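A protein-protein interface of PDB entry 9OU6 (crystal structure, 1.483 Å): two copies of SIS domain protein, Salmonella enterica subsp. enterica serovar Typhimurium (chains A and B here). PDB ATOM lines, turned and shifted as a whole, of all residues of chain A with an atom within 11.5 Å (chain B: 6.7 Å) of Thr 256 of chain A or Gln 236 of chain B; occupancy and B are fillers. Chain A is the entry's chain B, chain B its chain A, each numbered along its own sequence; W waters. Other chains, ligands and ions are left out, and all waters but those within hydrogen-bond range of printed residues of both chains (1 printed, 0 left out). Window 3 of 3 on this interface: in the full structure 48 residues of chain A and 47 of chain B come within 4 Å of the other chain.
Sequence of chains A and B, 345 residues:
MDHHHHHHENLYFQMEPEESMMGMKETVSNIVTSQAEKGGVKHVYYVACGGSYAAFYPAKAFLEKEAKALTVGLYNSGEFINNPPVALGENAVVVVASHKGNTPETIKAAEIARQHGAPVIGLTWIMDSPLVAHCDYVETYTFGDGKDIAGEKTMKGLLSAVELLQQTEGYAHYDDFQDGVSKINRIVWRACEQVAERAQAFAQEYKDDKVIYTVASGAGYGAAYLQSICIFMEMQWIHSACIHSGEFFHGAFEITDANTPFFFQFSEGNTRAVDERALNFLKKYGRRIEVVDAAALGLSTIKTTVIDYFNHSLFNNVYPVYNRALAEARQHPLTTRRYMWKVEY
Of chain B, only Phe 232 (3.9 Å), Gln 236 (3.2 Å) and Trp 237 (2.9 Å) come within 4 Å of Thr 256 of chain A. Printed residues of chain A within 4 Å of Gln 236 of chain B: Thr 256. Phe 232 of chain B touches just these residues of chain A: Glu 254 and Thr 256. No residue of chain A comes within 4 Å of Met 233 of chain B. Of the printed residues of chain A, Trp 237 of chain B touches Thr 256 (2.9 Å) and Ala 258 (3.6 Å). Printed residues of chain B within 4 Å of Tyr 213 of chain A: Ile 238 (3.5 Å). Of the printed residues of chain B, Ala 258 of chain A touches Trp 237. Printed residues of chain A within 4 Å of Ile 238 of chain B: Val 211, Tyr 213 and Ile 238. Printed residues of chain B within 4 Å of Ile 238 of chain A: Ile 238 (3.9 Å). The nearest residue of chain B that does not touch Thr 256 of chain A is Ile 238 of chain B (5.1 Å). The nearest residue of chain A that does not touch Gln 236 of chain B is Asp 257 of chain A (4.6 Å). The nearest printed residue of chain A that does not touch Ile 238 of chain B is Ser 240 of chain A (4.04 Å).
The backbone carbonyl oxygen (O) of Trp 237 of chain B lies within hydrogen-bond range of the side-chain hydroxyl (OG1) of Thr 256 of chain A, 2.9 Å away.
Ile 238 of chain A touches its own counterpart, Ile 238 of chain B. 1 position is printed for both chains.
The backbone NH (N) of Tyr 213 of chain A is in hydrogen-bond range of the backbone carbonyl oxygen (O) of Pro 261 of chain A, 3.0 Å away. O of Met 233 of chain B is in hydrogen-bond range of NE2 of Gln 236 of chain B (3.2 Å). OG1 of Thr 256 of chain A sits close to N of Ala 258 of chain A, at 3.2 Å.
Water W1 lies within hydrogen-bond range of OH of Tyr 213 of chain A (2.6 Å), O of Trp 237 of chain B (2.7 Å) and OG1 of Thr 260 of chain A (2.9 Å).
Hydrophobic or aromatic side chains of chain B within 4 Å of the printed part of chain A: Phe 232, Trp 237 and Ile 238. Of the 24 printed residues of chain A, 6 touch a printed residue of chain B. Hydrophobic or aromatic side chains of chain A that line the printed part of chain B: Val 211, Tyr 213, Ile 238 and Ala 258.
Among the printed residues, merely in contact across the chains: Thr 256 of chain A with Gln 236 of chain B (3.2 Å), Tyr 213 of chain A with Ile 238 of chain B (3.5 Å), Ala 258 of chain A with Trp 237 of chain B (3.6 Å), Glu 254 of chain A with Phe 232 of chain B (3.8 Å), Val 211 of chain A with Ile 238 of chain B (3.8 Å), Thr 256 of chain A with Phe 232 of chain B (3.9 Å) and Ile 238 of chain A with Ile 238 of chain B (3.9 Å).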
ATOM      1  N   ASP A 209       5.882  -7.072   0.332  1.00  0.00           N
ATOM      2  CA  ASP A 209       5.663  -6.302  -0.880  1.00  0.00           C
ATOM      3  C   ASP A 209       4.375  -6.741  -1.568  1.00  0.00           C
ATOM      4  O   ASP A 209       4.316  -7.839  -2.127  1.00  0.00           O
ATOM      5  CB  ASP A 209       6.821  -6.521  -1.832  1.00  0.00           C
ATOM      6  CG  ASP A 209       8.032  -5.654  -1.548  1.00  0.00           C
ATOM      7  OD1 ASP A 209       8.018  -4.508  -2.016  1.00  0.00           O
ATOM      8  OD2 ASP A 209       8.949  -6.116  -0.807  1.00  0.00           O
ATOM      9  N   VAL A 211       3.062  -5.651  -4.408  1.00  0.00           N
ATOM     10  CA  VAL A 211       3.074  -5.623  -5.863  1.00  0.00           C
ATOM     11  C   VAL A 211       4.516  -5.821  -6.305  1.00  0.00           C
ATOM     12  O   VAL A 211       5.446  -5.261  -5.720  1.00  0.00           O
ATOM     13  CB  VAL A 211       2.497  -4.275  -6.347  1.00  0.00           C
ATOM     14  CG1 VAL A 211       2.574  -4.117  -7.856  1.00  0.00           C
ATOM     15  CG2 VAL A 211       1.052  -4.097  -5.878  1.00  0.00           C
ATOM     16  N   ILE A 212       4.701  -6.610  -7.369  1.00  0.00           N
ATOM     17  CA  ILE A 212       6.012  -6.864  -7.938  1.00  0.00           C
ATOM     18  C   ILE A 212       5.850  -6.916  -9.459  1.00  0.00           C
ATOM     19  O   ILE A 212       5.027  -7.685  -9.956  1.00  0.00           O
ATOM     20  CB  ILE A 212       6.656  -8.173  -7.446  1.00  0.00           C
ATOM     21  CG1 ILE A 212       6.734  -8.285  -5.897  1.00  0.00           C
ATOM     22  CG2 ILE A 212       8.033  -8.323  -8.086  1.00  0.00           C
ATOM     23  CD1 ILE A 212       7.217  -9.631  -5.374  1.00  0.00           C
ATOM     24  N   TYR A 213       6.576  -6.075 -10.200  1.00  0.00           N
ATOM     25  CA  TYR A 213       6.545  -6.153 -11.650  1.00  0.00           C
ATOM     26  C   TYR A 213       7.393  -7.314 -12.146  1.00  0.00           C
ATOM     27  O   TYR A 213       8.426  -7.584 -11.592  1.00  0.00           O
ATOM     28  CB  TYR A 213       7.087  -4.893 -12.333  1.00  0.00           C
ATOM     29  CG  TYR A 213       6.288  -3.628 -12.178  1.00  0.00           C
ATOM     30  CD1 TYR A 213       5.053  -3.513 -12.775  1.00  0.00           C
ATOM     31  CD2 TYR A 213       6.804  -2.497 -11.548  1.00  0.00           C
ATOM     32  CE1 TYR A 213       4.331  -2.341 -12.703  1.00  0.00           C
ATOM     33  CE2 TYR A 213       6.072  -1.326 -11.446  1.00  0.00           C
ATOM     34  CZ  TYR A 213       4.845  -1.235 -12.047  1.00  0.00           C
ATOM     35  OH  TYR A 213       4.120  -0.089 -11.975  1.00  0.00           O
ATOM     36  N   ILE A 238      -2.817  -6.273  -6.412  1.00  0.00           N
ATOM     37  CA  ILE A 238      -3.028  -5.781  -7.782  1.00  0.00           C
ATOM     38  C   ILE A 238      -2.232  -6.664  -8.750  1.00  0.00           C
ATOM     39  O   ILE A 238      -1.080  -6.990  -8.473  1.00  0.00           O
ATOM     40  CB  ILE A 238      -2.562  -4.315  -7.870  1.00  0.00           C
ATOM     41  CG1 ILE A 238      -3.445  -3.386  -7.006  1.00  0.00           C
ATOM     42  CG2 ILE A 238      -2.455  -3.825  -9.323  1.00  0.00           C
ATOM     43  CD1 ILE A 238      -2.690  -2.178  -6.490  1.00  0.00           C
ATOM     44  N   SER A 240      -0.051  -6.517 -11.542  1.00  0.00           N
ATOM     45  CA  SER A 240       0.768  -5.509 -12.200  1.00  0.00           C
ATOM     46  C   SER A 240       1.252  -6.006 -13.560  1.00  0.00           C
ATOM     47  O   SER A 240       1.205  -7.201 -13.885  1.00  0.00           O
ATOM     48  CB  SER A 240       1.919  -5.076 -11.339  1.00  0.00           C
ATOM     49  OG  SER A 240       2.702  -6.196 -11.004  1.00  0.00           O
ATOM     50  N   ILE A 243       6.214  -6.357 -17.975  1.00  0.00           N
ATOM     51  CA  ILE A 243       6.798  -5.350 -18.848  1.00  0.00           C
ATOM     52  C   ILE A 243       7.742  -6.022 -19.822  1.00  0.00           C
ATOM     53  O   ILE A 243       8.693  -6.728 -19.429  1.00  0.00           O
ATOM     54  CB  ILE A 243       7.529  -4.287 -18.011  1.00  0.00           C
ATOM     55  CG1 ILE A 243       6.619  -3.715 -16.921  1.00  0.00           C
ATOM     56  CG2 ILE A 243       8.150  -3.197 -18.900  1.00  0.00           C
ATOM     57  CD1 ILE A 243       7.372  -3.091 -15.769  1.00  0.00           C
ATOM     58  N   PHE A 248      10.621  -0.126 -21.911  1.00  0.00           N
ATOM     59  CA  PHE A 248      10.925   0.755 -20.788  1.00  0.00           C
ATOM     60  C   PHE A 248      11.371   2.142 -21.240  1.00  0.00           C
ATOM     61  O   PHE A 248      11.480   3.083 -20.453  1.00  0.00           O
ATOM     62  CB  PHE A 248      12.214   0.356 -20.063  1.00  0.00           C
ATOM     63  CG  PHE A 248      11.979  -0.640 -18.954  1.00  0.00           C
ATOM     64  CD1 PHE A 248      11.449  -0.230 -17.742  1.00  0.00           C
ATOM     65  CD2 PHE A 248      12.247  -1.977 -19.147  1.00  0.00           C
ATOM     66  CE1 PHE A 248      11.252  -1.136 -16.716  1.00  0.00           C
ATOM     67  CE2 PHE A 248      12.006  -2.876 -18.134  1.00  0.00           C
ATOM     68  CZ  PHE A 248      11.517  -2.457 -16.923  1.00  0.00           C
ATOM     69  N   GLY A 251       7.311   3.928 -22.602  1.00  0.00           N
ATOM     70  CA  GLY A 251       5.963   3.914 -22.028  1.00  0.00           C
ATOM     71  C   GLY A 251       5.934   4.045 -20.514  1.00  0.00           C
ATOM     72  O   GLY A 251       4.963   3.517 -19.901  1.00  0.00           O
ATOM     73  N   GLU A 254       7.595   4.049 -15.841  1.00  0.00           N
ATOM     74  CA  GLU A 254       8.146   5.227 -15.123  1.00  0.00           C
ATOM     75  C   GLU A 254       8.376   4.850 -13.657  1.00  0.00           C
ATOM     76  O   GLU A 254       7.634   4.063 -13.081  1.00  0.00           O
ATOM     77  CB  GLU A 254       7.215   6.431 -15.267  1.00  0.00           C
ATOM     78  N   ILE A 255       9.415   5.407 -13.031  1.00  0.00           N
ATOM     79  CA  ILE A 255       9.609   5.192 -11.606  1.00  0.00           C
ATOM     80  C   ILE A 255       8.607   6.064 -10.860  1.00  0.00           C
ATOM     81  O   ILE A 255       8.582   7.271 -11.076  1.00  0.00           O
ATOM     82  CB  ILE A 255      11.053   5.524 -11.197  1.00  0.00           C
ATOM     83  CG1 ILE A 255      12.015   4.467 -11.722  1.00  0.00           C
ATOM     84  CG2 ILE A 255      11.165   5.726  -9.683  1.00  0.00           C
ATOM     85  CD1 ILE A 255      13.476   4.823 -11.548  1.00  0.00           C
ATOM     86  N   THR A 256       7.783   5.469  -9.986  1.00  0.00           N
ATOM     87  CA  THR A 256       6.900   6.281  -9.160  1.00  0.00           C
ATOM     88  C   THR A 256       7.253   6.126  -7.678  1.00  0.00           C
ATOM     89  O   THR A 256       8.131   5.350  -7.297  1.00  0.00           O
ATOM     90  CB  THR A 256       5.427   5.949  -9.412  1.00  0.00           C
ATOM     91  OG1 THR A 256       5.174   4.726  -8.717  1.00  0.00           O
ATOM     92  CG2 THR A 256       5.086   5.946 -10.896  1.00  0.00           C
ATOM     93  N   ASP A 257       6.520   6.893  -6.860  1.00  0.00           N
ATOM     94  CA  ASP A 257       6.626   6.868  -5.412  1.00  0.00           C
ATOM     95  C   ASP A 257       6.364   5.466  -4.860  1.00  0.00           C
ATOM     96  O   ASP A 257       6.874   5.139  -3.791  1.00  0.00           O
ATOM     97  CB  ASP A 257       5.703   7.901  -4.777  1.00  0.00           C
ATOM     98  CG  ASP A 257       6.161   9.352  -4.889  1.00  0.00           C
ATOM     99  OD1 ASP A 257       7.232   9.592  -5.492  1.00  0.00           O
ATOM    100  OD2 ASP A 257       5.446  10.236  -4.360  1.00  0.00           O
ATOM    101  N   ALA A 258       5.588   4.636  -5.583  1.00  0.00           N
ATOM    102  CA  ALA A 258       5.197   3.331  -5.072  1.00  0.00           C
ATOM    103  C   ALA A 258       6.419   2.458  -4.783  1.00  0.00           C
ATOM    104  O   ALA A 258       6.290   1.500  -4.030  1.00  0.00           O
ATOM    105  CB  ALA A 258       4.238   2.642  -6.042  1.00  0.00           C
ATOM    106  N   ASN A 259       7.583   2.776  -5.383  1.00  0.00           N
ATOM    107  CA  ASN A 259       8.833   2.042  -5.182  1.00  0.00           C
ATOM    108  C   ASN A 259       8.667   0.532  -5.426  1.00  0.00           C
ATOM    109  O   ASN A 259       9.260  -0.291  -4.739  1.00  0.00           O
ATOM    110  CB  ASN A 259       9.455   2.325  -3.818  1.00  0.00           C
ATOM    111  CG  ASN A 259      10.881   1.821  -3.728  1.00  0.00           C
ATOM    112  OD1 ASN A 259      11.284   1.240  -2.711  1.00  0.00           O
ATOM    113  ND2 ASN A 259      11.670   2.027  -4.772  1.00  0.00           N
ATOM    114  N   THR A 260       7.911   0.168  -6.464  1.00  0.00           N
ATOM    115  CA  THR A 260       7.622  -1.225  -6.749  1.00  0.00           C
ATOM    116  C   THR A 260       8.912  -1.982  -7.087  1.00  0.00           C
ATOM    117  O   THR A 260       9.712  -1.490  -7.873  1.00  0.00           O
ATOM    118  CB  THR A 260       6.631  -1.254  -7.915  1.00  0.00           C
ATOM    119  OG1 THR A 260       5.569  -0.323  -7.690  1.00  0.00           O
ATOM    120  CG2 THR A 260       6.023  -2.623  -8.112  1.00  0.00           C
ATOM    121  N   PRO A 261       9.158  -3.194  -6.552  1.00  0.00           N
ATOM    122  CA  PRO A 261      10.292  -3.994  -7.004  1.00  0.00           C
ATOM    123  C   PRO A 261      10.018  -4.754  -8.306  1.00  0.00           C
ATOM    124  O   PRO A 261       8.889  -4.735  -8.820  1.00  0.00           O
ATOM    125  CB  PRO A 261      10.544  -4.939  -5.851  1.00  0.00           C
ATOM    126  CG  PRO A 261       9.184  -5.083  -5.191  1.00  0.00           C
ATOM    127  CD  PRO A 261       8.358  -3.881  -5.534  1.00  0.00           C
ATOM    128  N   PHE A 262      11.089  -5.325  -8.864  1.00  0.00           N
ATOM    129  CA  PHE A 262      11.080  -6.022 -10.153  1.00  0.00           C
ATOM    130  C   PHE A 262      11.585  -7.450 -10.007  1.00  0.00           C
ATOM    131  O   PHE A 262      12.626  -7.682  -9.378  1.00  0.00           O
ATOM    132  CB  PHE A 262      11.968  -5.309 -11.175  1.00  0.00           C
ATOM    133  CG  PHE A 262      11.468  -3.902 -11.463  1.00  0.00           C
ATOM    134  CD1 PHE A 262      11.791  -2.846 -10.628  1.00  0.00           C
ATOM    135  CD2 PHE A 262      10.684  -3.643 -12.565  1.00  0.00           C
ATOM    136  CE1 PHE A 262      11.315  -1.571 -10.881  1.00  0.00           C
ATOM    137  CE2 PHE A 262      10.247  -2.368 -12.842  1.00  0.00           C
ATOM    138  CZ  PHE A 262      10.565  -1.325 -11.999  1.00  0.00           C
ATOM    139  N   PHE A 281      19.436  -0.109 -16.870  1.00  0.00           N
ATOM    140  CA  PHE A 281      18.629   1.033 -16.476  1.00  0.00           C
ATOM    141  C   PHE A 281      18.136   0.866 -15.046  1.00  0.00           C
ATOM    142  O   PHE A 281      18.214   1.816 -14.250  1.00  0.00           O
ATOM    143  CB  PHE A 281      17.469   1.182 -17.457  1.00  0.00           C
ATOM    144  CG  PHE A 281      16.342   2.061 -16.951  1.00  0.00           C
ATOM    145  CD1 PHE A 281      16.473   3.442 -16.946  1.00  0.00           C
ATOM    146  CD2 PHE A 281      15.116   1.509 -16.590  1.00  0.00           C
ATOM    147  CE1 PHE A 281      15.442   4.246 -16.524  1.00  0.00           C
ATOM    148  CE2 PHE A 281      14.076   2.321 -16.180  1.00  0.00           C
ATOM    149  CZ  PHE A 281      14.259   3.689 -16.101  1.00  0.00           C
ATOM    150  N   LEU A 282      17.552  -0.310 -14.712  1.00  0.00           N
ATOM    151  CA  LEU A 282      16.978  -0.487 -13.376  1.00  0.00           C
ATOM    152  C   LEU A 282      18.066  -0.374 -12.308  1.00  0.00           C
ATOM    153  O   LEU A 282      17.798   0.064 -11.185  1.00  0.00           O
ATOM    154  CB  LEU A 282      16.276  -1.839 -13.253  1.00  0.00           C
ATOM    155  CG  LEU A 282      15.063  -1.983 -14.172  1.00  0.00           C
ATOM    156  CD1 LEU A 282      14.647  -3.462 -14.281  1.00  0.00           C
ATOM    157  CD2 LEU A 282      13.907  -1.068 -13.685  1.00  0.00           C
ATOM    158  N   TYR A 285      19.126   3.295 -11.567  1.00  0.00           N
ATOM    159  CA  TYR A 285      18.219   4.027 -10.695  1.00  0.00           C
ATOM    160  C   TYR A 285      18.029   3.371  -9.337  1.00  0.00           C
ATOM    161  O   TYR A 285      17.088   3.734  -8.638  1.00  0.00           O
ATOM    162  CB  TYR A 285      16.871   4.219 -11.388  1.00  0.00           C
ATOM    163  CG  TYR A 285      16.950   5.300 -12.450  1.00  0.00           C
ATOM    164  CD1 TYR A 285      17.393   5.024 -13.727  1.00  0.00           C
ATOM    165  CD2 TYR A 285      16.620   6.622 -12.150  1.00  0.00           C
ATOM    166  CE1 TYR A 285      17.464   6.013 -14.697  1.00  0.00           C
ATOM    167  CE2 TYR A 285      16.713   7.618 -13.102  1.00  0.00           C
ATOM    168  CZ  TYR A 285      17.116   7.310 -14.389  1.00  0.00           C
ATOM    169  OH  TYR A 285      17.229   8.239 -15.391  1.00  0.00           O
ATOM    170  N   GLY A 286      18.847   2.373  -9.004  1.00  0.00           N
ATOM    171  CA  GLY A 286      18.872   1.792  -7.680  1.00  0.00           C
ATOM    172  C   GLY A 286      17.582   1.073  -7.323  1.00  0.00           C
ATOM    173  O   GLY A 286      17.172   1.054  -6.170  1.00  0.00           O
ATOM    174  N   ARG A 287      16.938   0.438  -8.314  1.00  0.00           N
ATOM    175  CA  ARG A 287      15.689  -0.238  -8.029  1.00  0.00           C
ATOM    176  C   ARG A 287      15.972  -1.542  -7.298  1.00  0.00           C
ATOM    177  O   ARG A 287      17.088  -2.075  -7.358  1.00  0.00           O
ATOM    178  CB  ARG A 287      14.915  -0.543  -9.323  1.00  0.00           C
ATOM    179  CG  ARG A 287      14.675   0.612 -10.281  1.00  0.00           C
ATOM    180  CD  ARG A 287      14.553   1.959  -9.606  1.00  0.00           C
ATOM    181  NE  ARG A 287      13.311   2.006  -8.857  1.00  0.00           N
ATOM    182  CZ  ARG A 287      13.027   2.920  -7.939  1.00  0.00           C
ATOM    183  NH1 ARG A 287      13.978   3.704  -7.453  1.00  0.00           N
ATOM    184  NH2 ARG A 287      11.791   3.005  -7.483  1.00  0.00           N
ATOM    185  N   ARG A 288      14.948  -2.047  -6.610  1.00  0.00           N
ATOM    186  CA  ARG A 288      15.001  -3.374  -6.000  1.00  0.00           C
ATOM    187  C   ARG A 288      14.655  -4.401  -7.079  1.00  0.00           C
ATOM    188  O   ARG A 288      13.578  -4.293  -7.663  1.00  0.00           O
ATOM    189  CB  ARG A 288      14.010  -3.435  -4.841  1.00  0.00           C
ATOM    190  CG  ARG A 288      14.402  -2.439  -3.749  1.00  0.00           C
ATOM    191  CD  ARG A 288      13.261  -2.273  -2.758  1.00  0.00           C
ATOM    192  NE  ARG A 288      12.965  -3.509  -2.030  1.00  0.00           N
ATOM    193  CZ  ARG A 288      11.733  -3.907  -1.750  1.00  0.00           C
ATOM    194  NH1 ARG A 288      10.701  -3.225  -2.199  1.00  0.00           N
ATOM    195  NH2 ARG A 288      11.526  -4.979  -1.012  1.00  0.00           N
ATOM    196  N   LYS B 210      -6.185   5.000  -7.515  1.00  0.00           N
ATOM    197  CA  LYS B 210      -4.803   5.021  -7.951  1.00  0.00           C
ATOM    198  C   LYS B 210      -4.499   3.895  -8.941  1.00  0.00           C
ATOM    199  O   LYS B 210      -3.552   4.032  -9.724  1.00  0.00           O
ATOM    200  CB  LYS B 210      -3.856   4.916  -6.750  1.00  0.00           C
ATOM    201  CG  LYS B 210      -4.165   5.916  -5.622  1.00  0.00           C
ATOM    202  CD  LYS B 210      -3.375   5.766  -4.327  1.00  0.00           C
ATOM    203  CE  LYS B 210      -1.903   5.936  -4.487  1.00  0.00           C
ATOM    204  NZ  LYS B 210      -1.554   7.103  -5.302  1.00  0.00           N
ATOM    205  N   ILE B 231      -3.748   5.841 -17.900  1.00  0.00           N
ATOM    206  CA  ILE B 231      -4.186   5.798 -16.514  1.00  0.00           C
ATOM    207  C   ILE B 231      -2.983   5.836 -15.576  1.00  0.00           C
ATOM    208  O   ILE B 231      -2.972   6.532 -14.544  1.00  0.00           O
ATOM    209  CB  ILE B 231      -5.035   4.551 -16.277  1.00  0.00           C
ATOM    210  CG1 ILE B 231      -6.427   4.707 -16.891  1.00  0.00           C
ATOM    211  CG2 ILE B 231      -5.079   4.238 -14.777  1.00  0.00           C
ATOM    212  CD1 ILE B 231      -7.179   3.375 -16.980  1.00  0.00           C
ATOM    213  N   PHE B 232      -1.974   5.039 -15.908  1.00  0.00           N
ATOM    214  CA  PHE B 232      -0.763   4.996 -15.111  1.00  0.00           C
ATOM    215  C   PHE B 232      -0.125   6.386 -15.038  1.00  0.00           C
ATOM    216  O   PHE B 232       0.338   6.778 -13.956  1.00  0.00           O
ATOM    217  CB  PHE B 232       0.192   3.987 -15.759  1.00  0.00           C
ATOM    218  CG  PHE B 232       1.534   3.850 -15.067  1.00  0.00           C
ATOM    219  CD1 PHE B 232       1.606   3.810 -13.684  1.00  0.00           C
ATOM    220  CD2 PHE B 232       2.699   3.737 -15.805  1.00  0.00           C
ATOM    221  CE1 PHE B 232       2.823   3.670 -13.041  1.00  0.00           C
ATOM    222  CE2 PHE B 232       3.921   3.615 -15.153  1.00  0.00           C
ATOM    223  CZ  PHE B 232       3.975   3.588 -13.777  1.00  0.00           C
ATOM    224  N   MET B 233      -0.054   7.072 -16.181  1.00  0.00           N
ATOM    225  CA  MET B 233       0.531   8.420 -16.274  1.00  0.00           C
ATOM    226  C   MET B 233      -0.216   9.442 -15.412  1.00  0.00           C
ATOM    227  O   MET B 233       0.414  10.302 -14.780  1.00  0.00           O
ATOM    228  CB  MET B 233       0.619   8.883 -17.731  1.00  0.00           C
ATOM    229  CG  MET B 233       1.622   8.113 -18.567  1.00  0.00           C
ATOM    230  SD  MET B 233       3.316   8.204 -17.962  1.00  0.00           S
ATOM    231  CE  MET B 233       3.419   7.071 -16.575  1.00  0.00           C
ATOM    232  N   GLU B 234      -1.540   9.330 -15.326  1.00  0.00           N
ATOM    233  CA  GLU B 234      -2.353  10.232 -14.527  1.00  0.00           C
ATOM    234  C   GLU B 234      -2.199   9.925 -13.041  1.00  0.00           C
ATOM    235  O   GLU B 234      -2.045  10.827 -12.210  1.00  0.00           O
ATOM    236  CB  GLU B 234      -3.826  10.074 -14.918  1.00  0.00           C
ATOM    237  CG  GLU B 234      -4.790  10.902 -14.074  1.00  0.00           C
ATOM    238  CD  GLU B 234      -4.477  12.388 -14.050  1.00  0.00           C
ATOM    239  OE1 GLU B 234      -4.180  12.968 -15.125  1.00  0.00           O
ATOM    240  OE2 GLU B 234      -4.520  12.942 -12.925  1.00  0.00           O
ATOM    241  N   MET B 235      -2.241   8.638 -12.704  1.00  0.00           N
ATOM    242  CA  MET B 235      -2.334   8.202 -11.324  1.00  0.00           C
ATOM    243  C   MET B 235      -0.948   8.041 -10.712  1.00  0.00           C
ATOM    244  O   MET B 235      -0.806   8.202  -9.500  1.00  0.00           O
ATOM    245  CB  MET B 235      -3.134   6.907 -11.199  1.00  0.00           C
ATOM    246  CG  MET B 235      -4.563   7.050 -11.582  1.00  0.00           C
ATOM    247  SD  MET B 235      -5.333   8.333 -10.569  1.00  0.00           S
ATOM    248  CE  MET B 235      -7.010   8.241 -11.195  1.00  0.00           C
ATOM    249  N   GLN B 236       0.058   7.769 -11.544  1.00  0.00           N
ATOM    250  CA  GLN B 236       1.455   7.783 -11.123  1.00  0.00           C
ATOM    251  C   GLN B 236       1.698   6.792  -9.986  1.00  0.00           C
ATOM    252  O   GLN B 236       2.452   7.085  -9.059  1.00  0.00           O
ATOM    253  CB  GLN B 236       1.891   9.168 -10.628  1.00  0.00           C
ATOM    254  CG  GLN B 236       1.862  10.263 -11.683  1.00  0.00           C
ATOM    255  CD  GLN B 236       2.959  10.135 -12.716  1.00  0.00           C
ATOM    256  OE1 GLN B 236       3.622   9.100 -12.856  1.00  0.00           O
ATOM    257  NE2 GLN B 236       3.142  11.201 -13.479  1.00  0.00           N
ATOM    258  N   TRP B 237       1.054   5.623 -10.025  1.00  0.00           N
ATOM    259  CA  TRP B 237       1.181   4.673  -8.943  1.00  0.00           C
ATOM    260  C   TRP B 237       1.719   3.331  -9.454  1.00  0.00           C
ATOM    261  O   TRP B 237       2.929   3.089  -9.375  1.00  0.00           O
ATOM    262  CB  TRP B 237      -0.144   4.541  -8.192  1.00  0.00           C
ATOM    263  CG  TRP B 237       0.023   3.925  -6.836  1.00  0.00           C
ATOM    264  CD1 TRP B 237      -0.516   2.758  -6.394  1.00  0.00           C
ATOM    265  CD2 TRP B 237       0.837   4.435  -5.752  1.00  0.00           C
ATOM    266  NE1 TRP B 237      -0.124   2.517  -5.104  1.00  0.00           N
ATOM    267  CE2 TRP B 237       0.711   3.521  -4.685  1.00  0.00           C
ATOM    268  CE3 TRP B 237       1.646   5.568  -5.579  1.00  0.00           C
ATOM    269  CZ2 TRP B 237       1.362   3.708  -3.465  1.00  0.00           C
ATOM    270  CZ3 TRP B 237       2.303   5.744  -4.378  1.00  0.00           C
ATOM    271  CH2 TRP B 237       2.170   4.819  -3.342  1.00  0.00           C
ATOM    272  N   ILE B 238       0.830   2.483 -10.001  1.00  0.00           N
ATOM    273  CA  ILE B 238       1.212   1.174 -10.526  1.00  0.00           C
ATOM    274  C   ILE B 238       0.568   0.987 -11.891  1.00  0.00           C
ATOM    275  O   ILE B 238      -0.619   1.294 -12.044  1.00  0.00           O
ATOM    276  CB  ILE B 238       0.747   0.063  -9.581  1.00  0.00           C
ATOM    277  CG1 ILE B 238       1.475   0.180  -8.230  1.00  0.00           C
ATOM    278  CG2 ILE B 238       0.923  -1.317 -10.227  1.00  0.00           C
ATOM    279  CD1 ILE B 238       0.746  -0.485  -7.087  1.00  0.00           C
ATOM    280  N   ARG B 330      -8.532  16.105 -10.738  1.00  0.00           N
ATOM    281  CA  ARG B 330      -7.400  15.903  -9.852  1.00  0.00           C
ATOM    282  C   ARG B 330      -6.554  17.187  -9.829  1.00  0.00           C
ATOM    283  O   ARG B 330      -5.405  17.073  -9.377  1.00  0.00           O
ATOM    284  CB  ARG B 330      -6.659  14.635 -10.311  1.00  0.00           C
ATOM    285  CG  ARG B 330      -7.482  13.376 -10.067  1.00  0.00           C
ATOM    286  CD  ARG B 330      -7.023  12.170 -10.883  1.00  0.00           C
ATOM    287  NE  ARG B 330      -5.580  12.002 -10.718  1.00  0.00           N
ATOM    288  CZ  ARG B 330      -5.016  11.504  -9.640  1.00  0.00           C
ATOM    289  NH1 ARG B 330      -3.707  11.475  -9.539  1.00  0.00           N
ATOM    290  NH2 ARG B 330      -5.766  11.007  -8.683  1.00  0.00           N
HETATM  291  O   HOH W   1       4.889   1.377  -9.922  1.00  0.00           O
